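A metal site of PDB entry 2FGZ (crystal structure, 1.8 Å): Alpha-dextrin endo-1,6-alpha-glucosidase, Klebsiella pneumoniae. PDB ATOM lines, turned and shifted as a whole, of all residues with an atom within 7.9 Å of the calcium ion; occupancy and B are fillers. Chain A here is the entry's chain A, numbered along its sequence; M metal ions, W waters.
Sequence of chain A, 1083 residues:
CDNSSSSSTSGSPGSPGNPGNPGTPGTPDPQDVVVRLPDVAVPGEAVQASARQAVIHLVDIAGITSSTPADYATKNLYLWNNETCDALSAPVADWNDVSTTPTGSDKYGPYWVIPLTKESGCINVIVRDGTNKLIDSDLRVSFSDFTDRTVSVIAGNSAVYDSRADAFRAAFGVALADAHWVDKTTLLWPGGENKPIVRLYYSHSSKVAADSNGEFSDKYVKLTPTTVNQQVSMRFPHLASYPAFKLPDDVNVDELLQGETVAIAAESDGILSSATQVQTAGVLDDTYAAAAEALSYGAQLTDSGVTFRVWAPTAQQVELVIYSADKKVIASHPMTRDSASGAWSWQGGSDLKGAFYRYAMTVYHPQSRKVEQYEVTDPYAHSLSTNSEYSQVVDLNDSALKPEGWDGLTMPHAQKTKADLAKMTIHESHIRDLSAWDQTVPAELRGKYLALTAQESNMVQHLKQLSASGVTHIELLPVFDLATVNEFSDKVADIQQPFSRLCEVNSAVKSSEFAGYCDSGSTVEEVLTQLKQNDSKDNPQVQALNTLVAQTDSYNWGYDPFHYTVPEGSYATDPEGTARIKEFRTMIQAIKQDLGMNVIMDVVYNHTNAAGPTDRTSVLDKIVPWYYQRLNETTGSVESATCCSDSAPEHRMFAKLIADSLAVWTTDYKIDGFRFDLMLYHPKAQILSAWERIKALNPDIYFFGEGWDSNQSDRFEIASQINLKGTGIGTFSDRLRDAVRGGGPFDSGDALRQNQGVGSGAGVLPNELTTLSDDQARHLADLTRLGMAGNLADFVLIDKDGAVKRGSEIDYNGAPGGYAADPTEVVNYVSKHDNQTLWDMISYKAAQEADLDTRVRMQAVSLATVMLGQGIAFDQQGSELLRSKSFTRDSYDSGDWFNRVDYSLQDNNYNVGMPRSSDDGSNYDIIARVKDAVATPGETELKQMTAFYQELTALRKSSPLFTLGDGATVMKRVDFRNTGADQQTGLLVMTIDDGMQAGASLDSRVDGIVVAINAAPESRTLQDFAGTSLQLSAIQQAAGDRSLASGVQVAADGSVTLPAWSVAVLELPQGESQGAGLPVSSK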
ATOM      1  N   THR A 484       9.657 -22.455  22.365  1.00  0.00           N
ATOM      2  CA  THR A 484       9.348 -23.030  23.670  1.00  0.00           C
ATOM      3  C   THR A 484       9.088 -24.527  23.852  1.00  0.00           C
ATOM      4  O   THR A 484       8.514 -24.945  24.858  1.00  0.00           O
ATOM      5  CB  THR A 484       8.183 -22.256  24.283  1.00  0.00           C
ATOM      6  OG1 THR A 484       7.153 -22.094  23.304  1.00  0.00           O
ATOM      7  CG2 THR A 484       8.661 -20.875  24.731  1.00  0.00           C
ATOM      8  N   VAL A 485       9.519 -25.316  22.882  1.00  0.00           N
ATOM      9  CA  VAL A 485       9.408 -26.771  22.970  1.00  0.00           C
ATOM     10  C   VAL A 485      10.744 -27.285  22.431  1.00  0.00           C
ATOM     11  O   VAL A 485      11.183 -26.855  21.355  1.00  0.00           O
ATOM     12  CB  VAL A 485       8.270 -27.350  22.106  1.00  0.00           C
ATOM     13  CG1 VAL A 485       8.389 -28.866  22.038  1.00  0.00           C
ATOM     14  CG2 VAL A 485       6.920 -26.972  22.692  1.00  0.00           C
ATOM     15  N   ASN A 486      11.388 -28.171  23.171  1.00  0.00           N
ATOM     16  CA  ASN A 486      12.669 -28.717  22.720  1.00  0.00           C
ATOM     17  C   ASN A 486      12.373 -29.778  21.675  1.00  0.00           C
ATOM     18  O   ASN A 486      11.623 -30.725  21.929  1.00  0.00           O
ATOM     19  CB  ASN A 486      13.434 -29.340  23.899  1.00  0.00           C
ATOM     20  CG  ASN A 486      14.899 -29.594  23.558  1.00  0.00           C
ATOM     21  OD1 ASN A 486      15.216 -30.084  22.476  1.00  0.00           O
ATOM     22  ND2 ASN A 486      15.788 -29.279  24.496  1.00  0.00           N
ATOM     23  N   ASP A 494       6.792 -36.471  28.355  1.00  0.00           N
ATOM     24  CA  ASP A 494       5.375 -36.145  28.336  1.00  0.00           C
ATOM     25  C   ASP A 494       4.653 -36.987  29.385  1.00  0.00           C
ATOM     26  O   ASP A 494       5.198 -37.971  29.874  1.00  0.00           O
ATOM     27  CB  ASP A 494       4.803 -36.369  26.931  1.00  0.00           C
ATOM     28  CG  ASP A 494       5.194 -35.237  25.974  1.00  0.00           C
ATOM     29  OD1 ASP A 494       4.764 -34.094  26.221  1.00  0.00           O
ATOM     30  OD2 ASP A 494       5.922 -35.491  24.999  1.00  0.00           O
ATOM     31  N   ASN A 546       2.181 -30.496  37.702  1.00  0.00           N
ATOM     32  CA  ASN A 546       2.078 -30.119  36.293  1.00  0.00           C
ATOM     33  C   ASN A 546       2.925 -28.912  35.924  1.00  0.00           C
ATOM     34  O   ASN A 546       3.428 -28.831  34.811  1.00  0.00           O
ATOM     35  CB  ASN A 546       0.624 -29.858  35.912  1.00  0.00           C
ATOM     36  CG  ASN A 546       0.400 -29.959  34.415  1.00  0.00           C
ATOM     37  OD1 ASN A 546       0.678 -31.000  33.818  1.00  0.00           O
ATOM     38  ND2 ASN A 546      -0.096 -28.896  33.799  1.00  0.00           N
ATOM     39  N   THR A 547       3.074 -27.977  36.847  1.00  0.00           N
ATOM     40  CA  THR A 547       3.874 -26.779  36.583  1.00  0.00           C
ATOM     41  C   THR A 547       5.313 -27.175  36.286  1.00  0.00           C
ATOM     42  O   THR A 547       5.988 -26.552  35.460  1.00  0.00           O
ATOM     43  CB  THR A 547       3.829 -25.811  37.781  1.00  0.00           C
ATOM     44  OG1 THR A 547       2.494 -25.315  37.930  1.00  0.00           O
ATOM     45  CG2 THR A 547       4.787 -24.646  37.569  1.00  0.00           C
ATOM     46  N   LEU A 548       5.791 -28.219  36.955  1.00  0.00           N
ATOM     47  CA  LEU A 548       7.140 -28.698  36.743  1.00  0.00           C
ATOM     48  C   LEU A 548       7.200 -29.477  35.426  1.00  0.00           C
ATOM     49  O   LEU A 548       8.140 -29.343  34.646  1.00  0.00           O
ATOM     50  CB  LEU A 548       7.559 -29.608  37.902  1.00  0.00           C
ATOM     51  CG  LEU A 548       7.526 -28.936  39.277  1.00  0.00           C
ATOM     52  CD1 LEU A 548       7.895 -29.950  40.357  1.00  0.00           C
ATOM     53  CD2 LEU A 548       8.503 -27.768  39.293  1.00  0.00           C
ATOM     54  N   VAL A 549       6.168 -30.274  35.176  1.00  0.00           N
ATOM     55  CA  VAL A 549       6.086 -31.058  33.953  1.00  0.00           C
ATOM     56  C   VAL A 549       6.139 -30.136  32.733  1.00  0.00           C
ATOM     57  O   VAL A 549       6.774 -30.454  31.733  1.00  0.00           O
ATOM     58  CB  VAL A 549       4.768 -31.887  33.902  1.00  0.00           C
ATOM     59  CG1 VAL A 549       4.592 -32.515  32.522  1.00  0.00           C
ATOM     60  CG2 VAL A 549       4.787 -32.970  34.989  1.00  0.00           C
ATOM     61  N   ALA A 550       5.466 -28.992  32.840  1.00  0.00           N
ATOM     62  CA  ALA A 550       5.396 -28.024  31.741  1.00  0.00           C
ATOM     63  C   ALA A 550       6.738 -27.541  31.217  1.00  0.00           C
ATOM     64  O   ALA A 550       6.846 -27.125  30.065  1.00  0.00           O
ATOM     65  CB  ALA A 550       4.555 -26.827  32.188  1.00  0.00           C
ATOM     66  N   GLN A 551       7.765 -27.577  32.066  1.00  0.00           N
ATOM     67  CA  GLN A 551       9.104 -27.129  31.691  1.00  0.00           C
ATOM     68  C   GLN A 551       9.797 -27.992  30.655  1.00  0.00           C
ATOM     69  O   GLN A 551      10.629 -27.497  29.884  1.00  0.00           O
ATOM     70  CB  GLN A 551       9.989 -27.043  32.932  1.00  0.00           C
ATOM     71  CG  GLN A 551       9.436 -26.175  34.048  1.00  0.00           C
ATOM     72  CD  GLN A 551      10.211 -26.327  35.346  1.00  0.00           C
ATOM     73  OE1 GLN A 551       9.936 -25.635  36.332  1.00  0.00           O
ATOM     74  NE2 GLN A 551      11.171 -27.235  35.357  1.00  0.00           N
ATOM     75  N   THR A 552       9.468 -29.280  30.630  1.00  0.00           N
ATOM     76  CA  THR A 552      10.122 -30.213  29.704  1.00  0.00           C
ATOM     77  C   THR A 552       9.198 -31.096  28.875  1.00  0.00           C
ATOM     78  O   THR A 552       9.638 -32.136  28.368  1.00  0.00           O
ATOM     79  CB  THR A 552      11.117 -31.102  30.483  1.00  0.00           C
ATOM     80  OG1 THR A 552      10.451 -31.661  31.633  1.00  0.00           O
ATOM     81  CG2 THR A 552      12.317 -30.291  30.959  1.00  0.00           C
ATOM     82  N   ASP A 553       7.935 -30.711  28.702  1.00  0.00           N
ATOM     83  CA  ASP A 553       7.024 -31.513  27.897  1.00  0.00           C
ATOM     84  C   ASP A 553       6.997 -31.013  26.444  1.00  0.00           C
ATOM     85  O   ASP A 553       7.754 -30.123  26.072  1.00  0.00           O
ATOM     86  CB  ASP A 553       5.606 -31.550  28.495  1.00  0.00           C
ATOM     87  CG  ASP A 553       4.951 -30.175  28.564  1.00  0.00           C
ATOM     88  OD1 ASP A 553       5.433 -29.227  27.907  1.00  0.00           O
ATOM     89  OD2 ASP A 553       3.929 -30.039  29.272  1.00  0.00           O
ATOM     90  N   SER A 554       6.119 -31.588  25.636  1.00  0.00           N
ATOM     91  CA  SER A 554       6.013 -31.188  24.232  1.00  0.00           C
ATOM     92  C   SER A 554       4.954 -30.120  24.026  1.00  0.00           C
ATOM     93  O   SER A 554       4.643 -29.765  22.887  1.00  0.00           O
ATOM     94  CB  SER A 554       5.649 -32.403  23.371  1.00  0.00           C
ATOM     95  OG  SER A 554       6.620 -33.437  23.437  1.00  0.00           O
ATOM     96  N   TYR A 555       4.420 -29.588  25.127  1.00  0.00           N
ATOM     97  CA  TYR A 555       3.325 -28.625  25.042  1.00  0.00           C
ATOM     98  C   TYR A 555       3.545 -27.128  25.225  1.00  0.00           C
ATOM     99  O   TYR A 555       4.174 -26.688  26.179  1.00  0.00           O
ATOM    100  CB  TYR A 555       2.214 -29.042  26.020  1.00  0.00           C
ATOM    101  CG  TYR A 555       0.897 -28.397  25.705  1.00  0.00           C
ATOM    102  CD1 TYR A 555       0.678 -27.042  25.964  1.00  0.00           C
ATOM    103  CD2 TYR A 555      -0.112 -29.115  25.063  1.00  0.00           C
ATOM    104  CE1 TYR A 555      -0.504 -26.425  25.567  1.00  0.00           C
ATOM    105  CE2 TYR A 555      -1.297 -28.506  24.660  1.00  0.00           C
ATOM    106  CZ  TYR A 555      -1.484 -27.150  24.920  1.00  0.00           C
ATOM    107  OH  TYR A 555      -2.633 -26.539  24.481  1.00  0.00           O
ATOM    108  N   ASN A 556       2.984 -26.364  24.293  1.00  0.00           N
ATOM    109  CA  ASN A 556       2.993 -24.903  24.334  1.00  0.00           C
ATOM    110  C   ASN A 556       2.183 -24.386  23.161  1.00  0.00           C
ATOM    111  O   ASN A 556       2.217 -24.962  22.073  1.00  0.00           O
ATOM    112  CB  ASN A 556       4.423 -24.338  24.261  1.00  0.00           C
ATOM    113  CG  ASN A 556       4.500 -22.908  24.793  1.00  0.00           C
ATOM    114  OD1 ASN A 556       3.975 -21.969  24.182  1.00  0.00           O
ATOM    115  ND2 ASN A 556       5.158 -22.738  25.932  1.00  0.00           N
ATOM    116  N   TRP A 557       1.404 -23.327  23.379  1.00  0.00           N
ATOM    117  CA  TRP A 557       0.619 -22.729  22.293  1.00  0.00           C
ATOM    118  C   TRP A 557       1.560 -22.343  21.165  1.00  0.00           C
ATOM    119  O   TRP A 557       1.211 -22.455  19.985  1.00  0.00           O
ATOM    120  CB  TRP A 557      -0.122 -21.483  22.765  1.00  0.00           C
ATOM    121  CG  TRP A 557      -1.339 -21.749  23.580  1.00  0.00           C
ATOM    122  CD1 TRP A 557      -1.991 -22.940  23.726  1.00  0.00           C
ATOM    123  CD2 TRP A 557      -2.066 -20.789  24.351  1.00  0.00           C
ATOM    124  NE1 TRP A 557      -3.083 -22.785  24.547  1.00  0.00           N
ATOM    125  CE2 TRP A 557      -3.153 -21.476  24.948  1.00  0.00           C
ATOM    126  CE3 TRP A 557      -1.908 -19.422  24.598  1.00  0.00           C
ATOM    127  CZ2 TRP A 557      -4.074 -20.838  25.774  1.00  0.00           C
ATOM    128  CZ3 TRP A 557      -2.830 -18.784  25.423  1.00  0.00           C
ATOM    129  CH2 TRP A 557      -3.903 -19.491  26.005  1.00  0.00           C
ATOM    130  N   TYR A 892      -1.602 -21.557  28.077  1.00  0.00           N
ATOM    131  CA  TYR A 892      -0.506 -21.683  27.114  1.00  0.00           C
ATOM    132  C   TYR A 892       0.587 -22.696  27.437  1.00  0.00           C
ATOM    133  O   TYR A 892       1.196 -23.272  26.530  1.00  0.00           O
ATOM    134  CB  TYR A 892       0.151 -20.318  26.875  1.00  0.00           C
ATOM    135  CG  TYR A 892       1.155 -19.902  27.915  1.00  0.00           C
ATOM    136  CD1 TYR A 892       0.739 -19.472  29.178  1.00  0.00           C
ATOM    137  CD2 TYR A 892       2.519 -19.939  27.650  1.00  0.00           C
ATOM    138  CE1 TYR A 892       1.670 -19.095  30.150  1.00  0.00           C
ATOM    139  CE2 TYR A 892       3.457 -19.559  28.599  1.00  0.00           C
ATOM    140  CZ  TYR A 892       3.026 -19.143  29.852  1.00  0.00           C
ATOM    141  OH  TYR A 892       3.961 -18.771  30.795  1.00  0.00           O
ATOM    142  N   ASP A 893       0.854 -22.908  28.721  1.00  0.00           N
ATOM    143  CA  ASP A 893       1.902 -23.831  29.137  1.00  0.00           C
ATOM    144  C   ASP A 893       1.351 -24.795  30.195  1.00  0.00           C
ATOM    145  O   ASP A 893       2.104 -25.328  31.003  1.00  0.00           O
ATOM    146  CB  ASP A 893       3.075 -23.040  29.723  1.00  0.00           C
ATOM    147  CG  ASP A 893       4.394 -23.802  29.673  1.00  0.00           C
ATOM    148  OD1 ASP A 893       5.380 -23.319  30.274  1.00  0.00           O
ATOM    149  OD2 ASP A 893       4.459 -24.870  29.028  1.00  0.00           O
ATOM    150  N   SER A 894       0.040 -25.008  30.159  1.00  0.00           N
ATOM    151  CA  SER A 894      -0.616 -25.899  31.120  1.00  0.00           C
ATOM    152  C   SER A 894      -0.643 -27.368  30.685  1.00  0.00           C
ATOM    153  O   SER A 894      -1.320 -28.192  31.309  1.00  0.00           O
ATOM    154  CB  SER A 894      -2.028 -25.411  31.438  1.00  0.00           C
ATOM    155  OG  SER A 894      -1.959 -24.215  32.194  1.00  0.00           O
ATOM    156  N   GLY A 895       0.088 -27.673  29.620  1.00  0.00           N
ATOM    157  CA  GLY A 895       0.211 -29.038  29.127  1.00  0.00           C
ATOM    158  C   GLY A 895      -1.002 -29.799  28.626  1.00  0.00           C
ATOM    159  O   GLY A 895      -2.094 -29.249  28.480  1.00  0.00           O
ATOM    160  N   ASP A 896      -0.778 -31.084  28.358  1.00  0.00           N
ATOM    161  CA  ASP A 896      -1.841 -31.964  27.869  1.00  0.00           C
ATOM    162  C   ASP A 896      -2.946 -32.107  28.916  1.00  0.00           C
ATOM    163  O   ASP A 896      -4.111 -32.275  28.576  1.00  0.00           O
ATOM    164  CB  ASP A 896      -1.319 -33.382  27.577  1.00  0.00           C
ATOM    165  CG  ASP A 896      -0.369 -33.431  26.395  1.00  0.00           C
ATOM    166  OD1 ASP A 896      -0.458 -32.584  25.481  1.00  0.00           O
ATOM    167  OD2 ASP A 896       0.463 -34.363  26.362  1.00  0.00           O
HETATM  168 CA    CA M   1       5.497 -26.765  28.054  1.00  0.00          CA
HETATM  169  O   HOH W   1       6.788 -24.790  27.130  1.00  0.00           O
HETATM  170  O   HOH W   2       3.318 -27.413  29.159  1.00  0.00           O
HETATM  171  O   HOH W   3       7.389 -27.477  26.794  1.00  0.00           O
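Four residues have an atom within 4 Å of the calcium ion: Ala 550, Asp 553, Tyr 555 and Asp 893. The nearest printed residue that does not touch the calcium ion is Asn 556 (4.5 Å).
The calcium ion is bound by the backbone carbonyl oxygen of Tyr 555, the side-chain carboxylate of Asp 893, water W3, the backbone carbonyl oxygen of Ala 550, the side-chain carboxylate of Asp 553, water W2 and water W1.
Water W3 lies within hydrogen-bond range of O of Asp 553 (2.8 Å) and O of Thr 484 (3.4 Å). Water W1 bridges O of Thr 484 (2.9 Å) and ND2 of Asn 556 (2.9 Å). Water W2 lies within hydrogen-bond range of OD2 of Asp 553 (2.7 Å), O of Asp 893 (3.0 Å) and N of Gly 895 (3.3 Å).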
